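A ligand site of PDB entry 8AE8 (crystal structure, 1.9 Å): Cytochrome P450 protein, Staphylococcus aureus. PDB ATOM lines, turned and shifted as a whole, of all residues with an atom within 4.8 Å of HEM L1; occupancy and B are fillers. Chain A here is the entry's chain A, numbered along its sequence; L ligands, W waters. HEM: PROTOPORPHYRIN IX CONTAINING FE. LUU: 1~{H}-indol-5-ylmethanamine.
Leu 76 touches HEM L1.
Ala 77 touches HEM L1 (CA to O1D, 3.7 Å).
Met 95 touches HEM L1.
Val 229 touches HEM L1.
Ala 232 touches HEM L1 (CB to CHD, 3.3 Å).
Ala 233 touches HEM L1 (CB to CMC, 3.5 Å).
Pro 236 touches HEM L1 (CG to C3B, 3.6 Å).
CD2 of Leu 273 touches CBB of HEM L1, 3.97 Å away.
Val 279 touches HEM L1.
CG2 of Ile 282 touches O1A of HEM L1 (3.3 Å).
Ser 343 touches HEM L1 (O to CMA, 3.1 Å).
CE1 of Phe 344 touches C2B of HEM L1, 3.5 Å away.
Gly 345 touches HEM L1 (N to CMA, 3.6 Å).
Val 348 touches HEM L1.
Thr 350 touches HEM L1 (O to CBD, 3.8 Å).
Val 352 touches HEM L1 (CG1 to CMD, 3.5 Å).
Gly 353 touches HEM L1.
CD2 of Phe 356 touches CMC of HEM L1 (3.9 Å).
OG of Ser 357 touches CHC of HEM L1, 3.2 Å away.
Hydrophobic or aromatic side chains that line HEM L1: Leu 76, His 84, Met 95, Val 229, Ala 232, Ala 233, Pro 236, Leu 273, Val 279, Ile 282, Phe 344, His 349, Val 352 and Phe 356.
24 residues have an atom within 4 Å of HEM L1: Leu 76, Ala 77, His 84, Lys 88, Met 95, Val 229, Ala 232, Ala 233, Pro 236, Leu 273, Val 279, Ile 282, Arg 284, Ser 343, Phe 344, Gly 345, Val 348, His 349, Thr 350, Cys 351, Val 352, Gly 353, Phe 356 and Ser 357.
FE of HEM L1 is bound by SG of Cys 351 (2.3 Å).
NE2 of His 84 is in hydrogen-bond range of O2D of HEM L1 (2.7 Å).
NH2 of Arg 284 is in salt-bridge range of O2A of HEM L1 (2.8 Å).
A ring nitrogen (ND1) of His 349 is in hydrogen-bond range of an oxygen (O1D) of HEM L1 (2.8 Å).
The side-chain amino group (NZ) of Lys 88 lies within salt-bridge range of an oxygen (O2D) of HEM L1 (3.0 Å).
The backbone carbonyl oxygen (O) of Ala 232 lies close to a nitrogen (N1) of LUU L2 (3.3 Å).
The backbone carbonyl oxygen (O) of Phe 344 is in hydrogen-bond range of the backbone NH (N) of Cys 351 (3.0 Å).
The backbone NH (N) of Gly 353 lies close to the side-chain sulfur (SG) of Cys 351, at 3.2 Å.
A ring nitrogen (NE2) of His 84 is in hydrogen-bond range of a ring nitrogen (ND1) of His 349, at 3.4 Å.
NZ of Lys 88 lies within hydrogen-bond range of O of Val 348, at 2.9 Å.
The backbone carbonyl oxygen (O) of Leu 273 sits at hydrogen-bond distance from the side-chain hydroxyl (OG) of Ser 343 (2.8 Å).
OG1 of Thr 350 is in hydrogen-bond range of O of Phe 344, 3.0 Å away.
N of Leu 76 sits at hydrogen-bond distance from OD1 of Asn 228 (3.5 Å).
The backbone carbonyl oxygen (O) of Pro 236 lies within hydrogen-bond range of the side-chain hydroxyl (OG1) of Thr 240.
N1 of LUU L2 binds FE of HEM L1 (2.3 Å).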
ATOM      1  N   LEU A  52      33.500 -11.831 -20.382  1.00  0.00           N
ATOM      2  CA  LEU A  52      32.462 -10.793 -20.383  1.00  0.00           C
ATOM      3  C   LEU A  52      33.000  -9.435 -19.941  1.00  0.00           C
ATOM      4  O   LEU A  52      32.449  -8.388 -20.323  1.00  0.00           O
ATOM      5  CB  LEU A  52      31.281 -11.216 -19.480  1.00  0.00           C
ATOM      6  CG  LEU A  52      30.578 -12.516 -19.864  1.00  0.00           C
ATOM      7  CD1 LEU A  52      29.589 -12.962 -18.795  1.00  0.00           C
ATOM      8  CD2 LEU A  52      29.886 -12.361 -21.214  1.00  0.00           C
ATOM      9  N   LEU A  63      26.583 -11.648 -32.214  1.00  0.00           N
ATOM     10  CA  LEU A  63      25.142 -11.423 -32.094  1.00  0.00           C
ATOM     11  C   LEU A  63      24.748 -10.283 -33.036  1.00  0.00           C
ATOM     12  O   LEU A  63      24.471  -9.156 -32.631  1.00  0.00           O
ATOM     13  CB  LEU A  63      24.777 -11.109 -30.655  1.00  0.00           C
ATOM     14  CG  LEU A  63      25.072 -12.225 -29.650  1.00  0.00           C
ATOM     15  CD1 LEU A  63      25.949 -11.715 -28.505  1.00  0.00           C
ATOM     16  CD2 LEU A  63      23.790 -12.840 -29.093  1.00  0.00           C
ATOM     17  N   LEU A  76      20.802  -3.253 -29.282  1.00  0.00           N
ATOM     18  CA  LEU A  76      21.709  -2.674 -28.290  1.00  0.00           C
ATOM     19  C   LEU A  76      23.047  -3.409 -28.243  1.00  0.00           C
ATOM     20  O   LEU A  76      24.107  -2.783 -28.175  1.00  0.00           O
ATOM     21  CB  LEU A  76      21.042  -2.686 -26.917  1.00  0.00           C
ATOM     22  CG  LEU A  76      21.732  -1.831 -25.843  1.00  0.00           C
ATOM     23  CD1 LEU A  76      21.615  -0.348 -26.133  1.00  0.00           C
ATOM     24  CD2 LEU A  76      21.187  -2.167 -24.451  1.00  0.00           C
ATOM     25  N   ALA A  77      23.013  -4.749 -28.294  1.00  0.00           N
ATOM     26  CA  ALA A  77      24.238  -5.515 -28.154  1.00  0.00           C
ATOM     27  C   ALA A  77      25.240  -5.163 -29.236  1.00  0.00           C
ATOM     28  O   ALA A  77      26.452  -5.216 -29.015  1.00  0.00           O
ATOM     29  CB  ALA A  77      23.949  -7.015 -28.189  1.00  0.00           C
ATOM     30  N   HIS A  84      26.086   3.159 -27.182  1.00  0.00           N
ATOM     31  CA  HIS A  84      25.542   2.081 -26.381  1.00  0.00           C
ATOM     32  C   HIS A  84      25.157   2.550 -24.992  1.00  0.00           C
ATOM     33  O   HIS A  84      24.101   2.150 -24.464  1.00  0.00           O
ATOM     34  CB  HIS A  84      26.534   0.926 -26.291  1.00  0.00           C
ATOM     35  CG  HIS A  84      26.207  -0.067 -25.226  1.00  0.00           C
ATOM     36  ND1 HIS A  84      26.742   0.003 -23.959  1.00  0.00           N
ATOM     37  CD2 HIS A  84      25.395  -1.150 -25.238  1.00  0.00           C
ATOM     38  CE1 HIS A  84      26.293  -1.023 -23.245  1.00  0.00           C
ATOM     39  NE2 HIS A  84      25.473  -1.727 -23.995  1.00  0.00           N
ATOM     40  N   LYS A  88      21.390   2.572 -23.825  1.00  0.00           N
ATOM     41  CA  LYS A  88      21.136   1.718 -22.676  1.00  0.00           C
ATOM     42  C   LYS A  88      20.480   2.519 -21.558  1.00  0.00           C
ATOM     43  O   LYS A  88      19.573   2.034 -20.883  1.00  0.00           O
ATOM     44  CB  LYS A  88      22.430   1.082 -22.186  1.00  0.00           C
ATOM     45  CG  LYS A  88      22.240   0.073 -21.057  1.00  0.00           C
ATOM     46  CD  LYS A  88      23.478  -0.840 -20.909  1.00  0.00           C
ATOM     47  CE  LYS A  88      23.237  -1.930 -19.882  1.00  0.00           C
ATOM     48  NZ  LYS A  88      24.419  -2.916 -19.909  1.00  0.00           N
ATOM     49  N   ILE A  91      16.740   3.132 -22.327  1.00  0.00           N
ATOM     50  CA  ILE A  91      15.899   1.979 -22.023  1.00  0.00           C
ATOM     51  C   ILE A  91      15.694   1.857 -20.519  1.00  0.00           C
ATOM     52  O   ILE A  91      14.592   1.579 -20.057  1.00  0.00           O
ATOM     53  CB  ILE A  91      16.504   0.701 -22.621  1.00  0.00           C
ATOM     54  CG1 ILE A  91      16.300   0.704 -24.123  1.00  0.00           C
ATOM     55  CG2 ILE A  91      15.927  -0.546 -22.009  1.00  0.00           C
ATOM     56  CD1 ILE A  91      17.167  -0.288 -24.859  1.00  0.00           C
ATOM     57  N   MET A  95      12.044   1.787 -17.009  1.00  0.00           N
ATOM     58  CA  MET A  95      11.800   0.863 -15.907  1.00  0.00           C
ATOM     59  C   MET A  95      12.399   1.398 -14.602  1.00  0.00           C
ATOM     60  O   MET A  95      12.600   0.638 -13.654  1.00  0.00           O
ATOM     61  CB  MET A  95      12.333  -0.525 -16.287  1.00  0.00           C
ATOM     62  CG  MET A  95      13.857  -0.684 -16.415  1.00  0.00           C
ATOM     63  SD  MET A  95      14.252  -2.160 -17.460  1.00  0.00           S
ATOM     64  CE  MET A  95      14.126  -1.435 -19.072  1.00  0.00           C
ATOM     65  N   LEU A 142       5.418  -2.450 -20.269  1.00  0.00           N
ATOM     66  CA  LEU A 142       6.661  -1.686 -20.266  1.00  0.00           C
ATOM     67  C   LEU A 142       6.800  -0.880 -21.545  1.00  0.00           C
ATOM     68  O   LEU A 142       7.142   0.310 -21.494  1.00  0.00           O
ATOM     69  CB  LEU A 142       7.841  -2.634 -20.116  1.00  0.00           C
ATOM     70  CG  LEU A 142       9.230  -2.047 -20.251  1.00  0.00           C
ATOM     71  CD1 LEU A 142       9.477  -1.010 -19.224  1.00  0.00           C
ATOM     72  CD2 LEU A 142      10.244  -3.190 -20.143  1.00  0.00           C
ATOM     73  N   ASN A 228      13.846  -5.666 -29.302  1.00  0.00           N
ATOM     74  CA  ASN A 228      14.908  -6.139 -28.420  1.00  0.00           C
ATOM     75  C   ASN A 228      14.406  -6.228 -26.982  1.00  0.00           C
ATOM     76  O   ASN A 228      14.668  -7.218 -26.299  1.00  0.00           O
ATOM     77  CB  ASN A 228      16.117  -5.195 -28.524  1.00  0.00           C
ATOM     78  CG  ASN A 228      17.334  -5.668 -27.678  1.00  0.00           C
ATOM     79  OD1 ASN A 228      18.319  -4.934 -27.523  1.00  0.00           O
ATOM     80  ND2 ASN A 228      17.284  -6.904 -27.203  1.00  0.00           N
ATOM     81  N   VAL A 229      13.690  -5.204 -26.518  1.00  0.00           N
ATOM     82  CA  VAL A 229      13.131  -5.244 -25.175  1.00  0.00           C
ATOM     83  C   VAL A 229      12.084  -6.351 -25.061  1.00  0.00           C
ATOM     84  O   VAL A 229      12.042  -7.089 -24.069  1.00  0.00           O
ATOM     85  CB  VAL A 229      12.557  -3.864 -24.814  1.00  0.00           C
ATOM     86  CG1 VAL A 229      11.616  -3.961 -23.604  1.00  0.00           C
ATOM     87  CG2 VAL A 229      13.690  -2.857 -24.558  1.00  0.00           C
ATOM     88  N   ALA A 232      13.856  -9.627 -24.861  1.00  0.00           N
ATOM     89  CA  ALA A 232      14.738  -9.743 -23.711  1.00  0.00           C
ATOM     90  C   ALA A 232      13.957  -9.891 -22.415  1.00  0.00           C
ATOM     91  O   ALA A 232      14.379 -10.624 -21.516  1.00  0.00           O
ATOM     92  CB  ALA A 232      15.644  -8.526 -23.636  1.00  0.00           C
ATOM     93  N   ALA A 233      12.853  -9.171 -22.277  1.00  0.00           N
ATOM     94  CA  ALA A 233      12.130  -9.183 -21.019  1.00  0.00           C
ATOM     95  C   ALA A 233      11.195 -10.392 -20.888  1.00  0.00           C
ATOM     96  O   ALA A 233      10.938 -10.837 -19.775  1.00  0.00           O
ATOM     97  CB  ALA A 233      11.321  -7.905 -20.845  1.00  0.00           C
ATOM     98  N   PRO A 236      12.958 -14.835 -20.128  1.00  0.00           N
ATOM     99  CA  PRO A 236      13.465 -15.339 -18.839  1.00  0.00           C
ATOM    100  C   PRO A 236      12.511 -15.250 -17.676  1.00  0.00           C
ATOM    101  O   PRO A 236      12.767 -15.921 -16.676  1.00  0.00           O
ATOM    102  CB  PRO A 236      14.704 -14.469 -18.558  1.00  0.00           C
ATOM    103  CG  PRO A 236      14.758 -13.410 -19.618  1.00  0.00           C
ATOM    104  CD  PRO A 236      13.542 -13.549 -20.519  1.00  0.00           C
ATOM    105  N   THR A 240      11.928 -18.295 -14.752  1.00  0.00           N
ATOM    106  CA  THR A 240      12.477 -18.077 -13.425  1.00  0.00           C
ATOM    107  C   THR A 240      11.386 -18.204 -12.374  1.00  0.00           C
ATOM    108  O   THR A 240      11.620 -18.750 -11.295  1.00  0.00           O
ATOM    109  CB  THR A 240      13.137 -16.696 -13.328  1.00  0.00           C
ATOM    110  OG1 THR A 240      14.227 -16.600 -14.250  1.00  0.00           O
ATOM    111  CG2 THR A 240      13.697 -16.469 -11.974  1.00  0.00           C
ATOM    112  N   LEU A 273      18.182 -17.803  -9.776  1.00  0.00           N
ATOM    113  CA  LEU A 273      18.866 -17.388 -10.991  1.00  0.00           C
ATOM    114  C   LEU A 273      20.243 -18.059 -11.088  1.00  0.00           C
ATOM    115  O   LEU A 273      20.641 -18.440 -12.192  1.00  0.00           O
ATOM    116  CB  LEU A 273      18.961 -15.856 -11.031  1.00  0.00           C
ATOM    117  CG  LEU A 273      17.572 -15.241 -11.325  1.00  0.00           C
ATOM    118  CD1 LEU A 273      17.577 -13.734 -11.083  1.00  0.00           C
ATOM    119  CD2 LEU A 273      17.093 -15.538 -12.728  1.00  0.00           C
ATOM    120  N   PRO A 278      18.288 -19.101 -16.347  1.00  0.00           N
ATOM    121  CA  PRO A 278      17.326 -19.241 -17.456  1.00  0.00           C
ATOM    122  C   PRO A 278      17.942 -18.835 -18.779  1.00  0.00           C
ATOM    123  O   PRO A 278      17.532 -19.331 -19.831  1.00  0.00           O
ATOM    124  CB  PRO A 278      16.162 -18.296 -17.098  1.00  0.00           C
ATOM    125  CG  PRO A 278      16.578 -17.552 -15.852  1.00  0.00           C
ATOM    126  CD  PRO A 278      17.894 -18.120 -15.322  1.00  0.00           C
ATOM    127  N   VAL A 279      18.916 -17.929 -18.774  1.00  0.00           N
ATOM    128  CA  VAL A 279      19.743 -17.665 -19.944  1.00  0.00           C
ATOM    129  C   VAL A 279      21.034 -18.449 -19.760  1.00  0.00           C
ATOM    130  O   VAL A 279      21.822 -18.148 -18.869  1.00  0.00           O
ATOM    131  CB  VAL A 279      20.021 -16.160 -20.103  1.00  0.00           C
ATOM    132  CG1 VAL A 279      20.889 -15.910 -21.338  1.00  0.00           C
ATOM    133  CG2 VAL A 279      18.693 -15.385 -20.197  1.00  0.00           C
ATOM    134  N   ILE A 282      25.922 -17.209 -23.509  1.00  0.00           N
ATOM    135  CA  ILE A 282      26.214 -15.883 -24.038  1.00  0.00           C
ATOM    136  C   ILE A 282      27.384 -15.971 -25.023  1.00  0.00           C
ATOM    137  O   ILE A 282      28.518 -16.231 -24.611  1.00  0.00           O
ATOM    138  CB  ILE A 282      26.560 -14.899 -22.923  1.00  0.00           C
ATOM    139  CG1 ILE A 282      25.430 -14.801 -21.897  1.00  0.00           C
ATOM    140  CG2 ILE A 282      26.814 -13.514 -23.498  1.00  0.00           C
ATOM    141  CD1 ILE A 282      25.785 -13.861 -20.733  1.00  0.00           C
ATOM    142  N   ARG A 284      30.304 -14.653 -27.757  1.00  0.00           N
ATOM    143  CA  ARG A 284      31.197 -13.547 -28.073  1.00  0.00           C
ATOM    144  C   ARG A 284      32.091 -13.957 -29.227  1.00  0.00           C
ATOM    145  O   ARG A 284      32.339 -15.147 -29.466  1.00  0.00           O
ATOM    146  CB  ARG A 284      32.061 -13.095 -26.887  1.00  0.00           C
ATOM    147  CG  ARG A 284      31.298 -12.476 -25.733  1.00  0.00           C
ATOM    148  CD  ARG A 284      30.713 -11.121 -26.107  1.00  0.00           C
ATOM    149  NE  ARG A 284      30.184 -10.392 -24.947  1.00  0.00           N
ATOM    150  CZ  ARG A 284      28.900 -10.361 -24.603  1.00  0.00           C
ATOM    151  NH1 ARG A 284      27.985 -11.020 -25.292  1.00  0.00           N
ATOM    152  NH2 ARG A 284      28.525  -9.651 -23.540  1.00  0.00           N
ATOM    153  N   LEU A 342      26.476 -14.892 -12.404  1.00  0.00           N
ATOM    154  CA  LEU A 342      26.573 -14.325 -13.748  1.00  0.00           C
ATOM    155  C   LEU A 342      25.277 -14.430 -14.537  1.00  0.00           C
ATOM    156  O   LEU A 342      25.303 -14.325 -15.767  1.00  0.00           O
ATOM    157  CB  LEU A 342      27.692 -15.017 -14.520  1.00  0.00           C
ATOM    158  CG  LEU A 342      29.048 -14.794 -13.883  1.00  0.00           C
ATOM    159  CD1 LEU A 342      30.068 -15.842 -14.385  1.00  0.00           C
ATOM    160  CD2 LEU A 342      29.565 -13.408 -14.167  1.00  0.00           C
ATOM    161  N   SER A 343      24.150 -14.621 -13.850  1.00  0.00           N
ATOM    162  CA  SER A 343      22.851 -14.820 -14.515  1.00  0.00           C
ATOM    163  C   SER A 343      22.379 -13.622 -15.325  1.00  0.00           C
ATOM    164  O   SER A 343      21.618 -13.793 -16.281  1.00  0.00           O
ATOM    165  CB  SER A 343      21.784 -15.144 -13.472  1.00  0.00           C
ATOM    166  OG  SER A 343      22.241 -16.196 -12.639  1.00  0.00           O
ATOM    167  N   PHE A 344      22.769 -12.412 -14.915  1.00  0.00           N
ATOM    168  CA  PHE A 344      22.523 -11.187 -15.645  1.00  0.00           C
ATOM    169  C   PHE A 344      23.764 -10.739 -16.445  1.00  0.00           C
ATOM    170  O   PHE A 344      23.824  -9.612 -16.928  1.00  0.00           O
ATOM    171  CB  PHE A 344      22.140 -10.097 -14.651  1.00  0.00           C
ATOM    172  CG  PHE A 344      20.794 -10.281 -14.052  1.00  0.00           C
ATOM    173  CD1 PHE A 344      19.634 -10.256 -14.839  1.00  0.00           C
ATOM    174  CD2 PHE A 344      20.647 -10.401 -12.681  1.00  0.00           C
ATOM    175  CE1 PHE A 344      18.317 -10.407 -14.278  1.00  0.00           C
ATOM    176  CE2 PHE A 344      19.339 -10.498 -12.097  1.00  0.00           C
ATOM    177  CZ  PHE A 344      18.172 -10.515 -12.912  1.00  0.00           C
ATOM    178  N   GLY A 345      24.757 -11.615 -16.581  1.00  0.00           N
ATOM    179  CA  GLY A 345      25.951 -11.176 -17.261  1.00  0.00           C
ATOM    180  C   GLY A 345      26.779 -10.274 -16.358  1.00  0.00           C
ATOM    181  O   GLY A 345      26.558 -10.175 -15.147  1.00  0.00           O
ATOM    182  N   VAL A 348      30.229  -4.610 -19.831  1.00  0.00           N
ATOM    183  CA  VAL A 348      29.568  -3.541 -20.595  1.00  0.00           C
ATOM    184  C   VAL A 348      28.120  -3.901 -20.887  1.00  0.00           C
ATOM    185  O   VAL A 348      27.219  -3.068 -20.735  1.00  0.00           O
ATOM    186  CB  VAL A 348      30.352  -3.265 -21.884  1.00  0.00           C
ATOM    187  CG1 VAL A 348      29.508  -2.472 -22.864  1.00  0.00           C
ATOM    188  CG2 VAL A 348      31.667  -2.533 -21.593  1.00  0.00           C
ATOM    189  N   HIS A 349      27.869  -5.135 -21.321  1.00  0.00           N
ATOM    190  CA  HIS A 349      26.541  -5.496 -21.793  1.00  0.00           C
ATOM    191  C   HIS A 349      25.705  -6.215 -20.736  1.00  0.00           C
ATOM    192  O   HIS A 349      24.776  -6.964 -21.063  1.00  0.00           O
ATOM    193  CB  HIS A 349      26.615  -6.344 -23.064  1.00  0.00           C
ATOM    194  CG  HIS A 349      27.213  -5.617 -24.232  1.00  0.00           C
ATOM    195  ND1 HIS A 349      26.452  -4.833 -25.087  1.00  0.00           N
ATOM    196  CD2 HIS A 349      28.478  -5.552 -24.693  1.00  0.00           C
ATOM    197  CE1 HIS A 349      27.245  -4.305 -26.007  1.00  0.00           C
ATOM    198  NE2 HIS A 349      28.470  -4.727 -25.798  1.00  0.00           N
ATOM    199  N   THR A 350      26.003  -5.989 -19.458  1.00  0.00           N
ATOM    200  CA  THR A 350      25.210  -6.593 -18.406  1.00  0.00           C
ATOM    201  C   THR A 350      23.734  -6.180 -18.518  1.00  0.00           C
ATOM    202  O   THR A 350      23.402  -5.062 -18.922  1.00  0.00           O
ATOM    203  CB  THR A 350      25.758  -6.201 -17.022  1.00  0.00           C
ATOM    204  OG1 THR A 350      25.147  -7.041 -16.029  1.00  0.00           O
ATOM    205  CG2 THR A 350      25.442  -4.765 -16.716  1.00  0.00           C
ATOM    206  N   CYS A 351      22.853  -7.095 -18.138  1.00  0.00           N
ATOM    207  CA  CYS A 351      21.425  -6.898 -18.383  1.00  0.00           C
ATOM    208  C   CYS A 351      20.883  -5.573 -17.845  1.00  0.00           C
ATOM    209  O   CYS A 351      20.927  -5.309 -16.636  1.00  0.00           O
ATOM    210  CB  CYS A 351      20.613  -8.043 -17.791  1.00  0.00           C
ATOM    211  SG  CYS A 351      18.870  -7.777 -17.993  1.00  0.00           S
ATOM    212  N   VAL A 352      20.325  -4.748 -18.725  1.00  0.00           N
ATOM    213  CA  VAL A 352      19.807  -3.474 -18.258  1.00  0.00           C
ATOM    214  C   VAL A 352      18.583  -3.650 -17.382  1.00  0.00           C
ATOM    215  O   VAL A 352      18.267  -2.787 -16.555  1.00  0.00           O
ATOM    216  CB  VAL A 352      19.495  -2.558 -19.461  1.00  0.00           C
ATOM    217  CG1 VAL A 352      18.270  -3.151 -20.238  1.00  0.00           C
ATOM    218  CG2 VAL A 352      19.135  -1.150 -18.989  1.00  0.00           C
ATOM    219  N   GLY A 353      17.874  -4.762 -17.554  1.00  0.00           N
ATOM    220  CA  GLY A 353      16.661  -5.086 -16.853  1.00  0.00           C
ATOM    221  C   GLY A 353      16.815  -5.841 -15.552  1.00  0.00           C
ATOM    222  O   GLY A 353      15.802  -6.279 -15.002  1.00  0.00           O
ATOM    223  N   PHE A 356      14.895  -4.209 -12.394  1.00  0.00           N
ATOM    224  CA  PHE A 356      13.448  -4.327 -12.634  1.00  0.00           C
ATOM    225  C   PHE A 356      13.008  -5.783 -12.530  1.00  0.00           C
ATOM    226  O   PHE A 356      11.969  -6.070 -11.913  1.00  0.00           O
ATOM    227  CB  PHE A 356      13.113  -3.741 -14.011  1.00  0.00           C
ATOM    228  CG  PHE A 356      11.736  -4.032 -14.473  1.00  0.00           C
ATOM    229  CD1 PHE A 356      10.647  -3.485 -13.840  1.00  0.00           C
ATOM    230  CD2 PHE A 356      11.532  -4.848 -15.549  1.00  0.00           C
ATOM    231  CE1 PHE A 356       9.365  -3.757 -14.282  1.00  0.00           C
ATOM    232  CE2 PHE A 356      10.237  -5.130 -15.986  1.00  0.00           C
ATOM    233  CZ  PHE A 356       9.160  -4.576 -15.348  1.00  0.00           C
ATOM    234  N   SER A 357      13.787  -6.716 -13.081  1.00  0.00           N
ATOM    235  CA  SER A 357      13.437  -8.132 -13.004  1.00  0.00           C
ATOM    236  C   SER A 357      13.306  -8.583 -11.554  1.00  0.00           C
ATOM    237  O   SER A 357      12.353  -9.291 -11.198  1.00  0.00           O
ATOM    238  CB  SER A 357      14.474  -8.982 -13.729  1.00  0.00           C
ATOM    239  OG  SER A 357      14.302  -8.834 -15.117  1.00  0.00           O
ATOM    240  N   LEU A 361       9.762  -9.805 -10.110  1.00  0.00           N
ATOM    241  CA  LEU A 361       9.635 -11.186  -9.648  1.00  0.00           C
ATOM    242  C   LEU A 361       9.275 -11.217  -8.169  1.00  0.00           C
ATOM    243  O   LEU A 361       8.513 -12.078  -7.732  1.00  0.00           O
ATOM    244  CB  LEU A 361      10.926 -11.968  -9.895  1.00  0.00           C
ATOM    245  CG  LEU A 361      11.182 -12.328 -11.365  1.00  0.00           C
ATOM    246  CD1 LEU A 361      12.631 -12.743 -11.558  1.00  0.00           C
ATOM    247  CD2 LEU A 361      10.205 -13.433 -11.846  1.00  0.00           C
HETATM  248  CHA HEM L   1      21.168  -8.515 -21.515  1.00  0.00           C
HETATM  249  CHB HEM L   1      19.618 -12.033 -18.534  1.00  0.00           C
HETATM  250  CHC HEM L   1      15.526  -9.591 -17.965  1.00  0.00           C
HETATM  251  CHD HEM L   1      16.776  -6.474 -21.364  1.00  0.00           C
HETATM  252  C1A HEM L   1      21.162  -9.655 -20.728  1.00  0.00           C
HETATM  253  C2A HEM L   1      22.253 -10.576 -20.503  1.00  0.00           C
HETATM  254  C3A HEM L   1      21.799 -11.546 -19.682  1.00  0.00           C
HETATM  255  C4A HEM L   1      20.432 -11.258 -19.345  1.00  0.00           C
HETATM  256  CMA HEM L   1      22.518 -12.787 -19.107  1.00  0.00           C
HETATM  257  CAA HEM L   1      23.672 -10.434 -21.109  1.00  0.00           C
HETATM  258  CBA HEM L   1      23.697 -10.783 -22.592  1.00  0.00           C
HETATM  259  CGA HEM L   1      25.086 -10.577 -23.156  1.00  0.00           C
HETATM  260  O1A HEM L   1      25.238 -10.779 -24.382  1.00  0.00           O
HETATM  261  O2A HEM L   1      26.029 -10.194 -22.419  1.00  0.00           O
HETATM  262  C1B HEM L   1      18.371 -11.672 -18.078  1.00  0.00           C
HETATM  263  C2B HEM L   1      17.576 -12.352 -17.078  1.00  0.00           C
HETATM  264  C3B HEM L   1      16.433 -11.675 -16.929  1.00  0.00           C
HETATM  265  C4B HEM L   1      16.493 -10.546 -17.843  1.00  0.00           C
HETATM  266  CMB HEM L   1      18.003 -13.643 -16.341  1.00  0.00           C
HETATM  267  CAB HEM L   1      15.240 -11.937 -15.986  1.00  0.00           C
HETATM  268  CBB HEM L   1      15.308 -12.785 -14.958  1.00  0.00           C
HETATM  269  C1C HEM L   1      15.494  -8.490 -18.771  1.00  0.00           C
HETATM  270  C2C HEM L   1      14.474  -7.467 -18.797  1.00  0.00           C
HETATM  271  C3C HEM L   1      14.775  -6.583 -19.745  1.00  0.00           C
HETATM  272  C4C HEM L   1      16.023  -7.034 -20.355  1.00  0.00           C
HETATM  273  CMC HEM L   1      13.216  -7.432 -17.886  1.00  0.00           C
HETATM  274  CAC HEM L   1      13.900  -5.344 -20.037  1.00  0.00           C
HETATM  275  CBC HEM L   1      14.066  -4.624 -21.141  1.00  0.00           C
HETATM  276  C1D HEM L   1      18.096  -6.732 -21.674  1.00  0.00           C
HETATM  277  C2D HEM L   1      18.915  -5.958 -22.592  1.00  0.00           C
HETATM  278  C3D HEM L   1      20.113  -6.538 -22.653  1.00  0.00           C
HETATM  279  C4D HEM L   1      20.103  -7.679 -21.759  1.00  0.00           C
HETATM  280  CMD HEM L   1      18.504  -4.708 -23.396  1.00  0.00           C
HETATM  281  CAD HEM L   1      21.317  -6.033 -23.500  1.00  0.00           C
HETATM  282  CBD HEM L   1      22.319  -5.339 -22.560  1.00  0.00           C
HETATM  283  CGD HEM L   1      23.424  -4.630 -23.329  1.00  0.00           C
HETATM  284  O1D HEM L   1      23.707  -5.037 -24.479  1.00  0.00           O
HETATM  285  O2D HEM L   1      24.004  -3.629 -22.805  1.00  0.00           O
HETATM  286  NA  HEM L   1      20.086 -10.115 -20.021  1.00  0.00           N
HETATM  287  NB  HEM L   1      17.696 -10.541 -18.507  1.00  0.00           N
HETATM  288  NC  HEM L   1      16.378  -8.198 -19.739  1.00  0.00           N
HETATM  289  ND  HEM L   1      18.854  -7.786 -21.173  1.00  0.00           N
HETATM  290 FE   HEM L   1      18.245  -9.107 -19.751  1.00  0.00          FE
HETATM  291  C7  LUU L   2      16.003 -14.264 -25.686  1.00  0.00           C
HETATM  292  C2  LUU L   2      17.787 -12.636 -22.723  1.00  0.00           C
HETATM  293  C3  LUU L   2      19.080 -13.018 -23.149  1.00  0.00           C
HETATM  294  C4  LUU L   2      19.293 -13.750 -24.305  1.00  0.00           C
HETATM  295  C5  LUU L   2      18.185 -14.095 -25.068  1.00  0.00           C
HETATM  296  C6  LUU L   2      16.784 -14.893 -26.604  1.00  0.00           C
HETATM  297  C1  LUU L   2      17.602 -11.836 -21.451  1.00  0.00           C
HETATM  298  C8  LUU L   2      16.879 -13.737 -24.685  1.00  0.00           C
HETATM  299  C9  LUU L   2      16.687 -12.997 -23.502  1.00  0.00           C
HETATM  300  N1  LUU L   2      17.679 -10.376 -21.630  1.00  0.00           N
HETATM  301  N2  LUU L   2      18.097 -14.803 -26.239  1.00  0.00           N
HETATM  302  O   HOH W   1      23.620  -7.857 -25.382  1.00  0.00           O
HETATM  303  O   HOH W   2      23.253 -11.930 -25.726  1.00  0.00           O
HETATM  304  O   HOH W   3      27.108  -9.516 -19.921  1.00  0.00           O
HETATM  305  O   HOH W   4      12.071  -9.605 -16.007  1.00  0.00           O
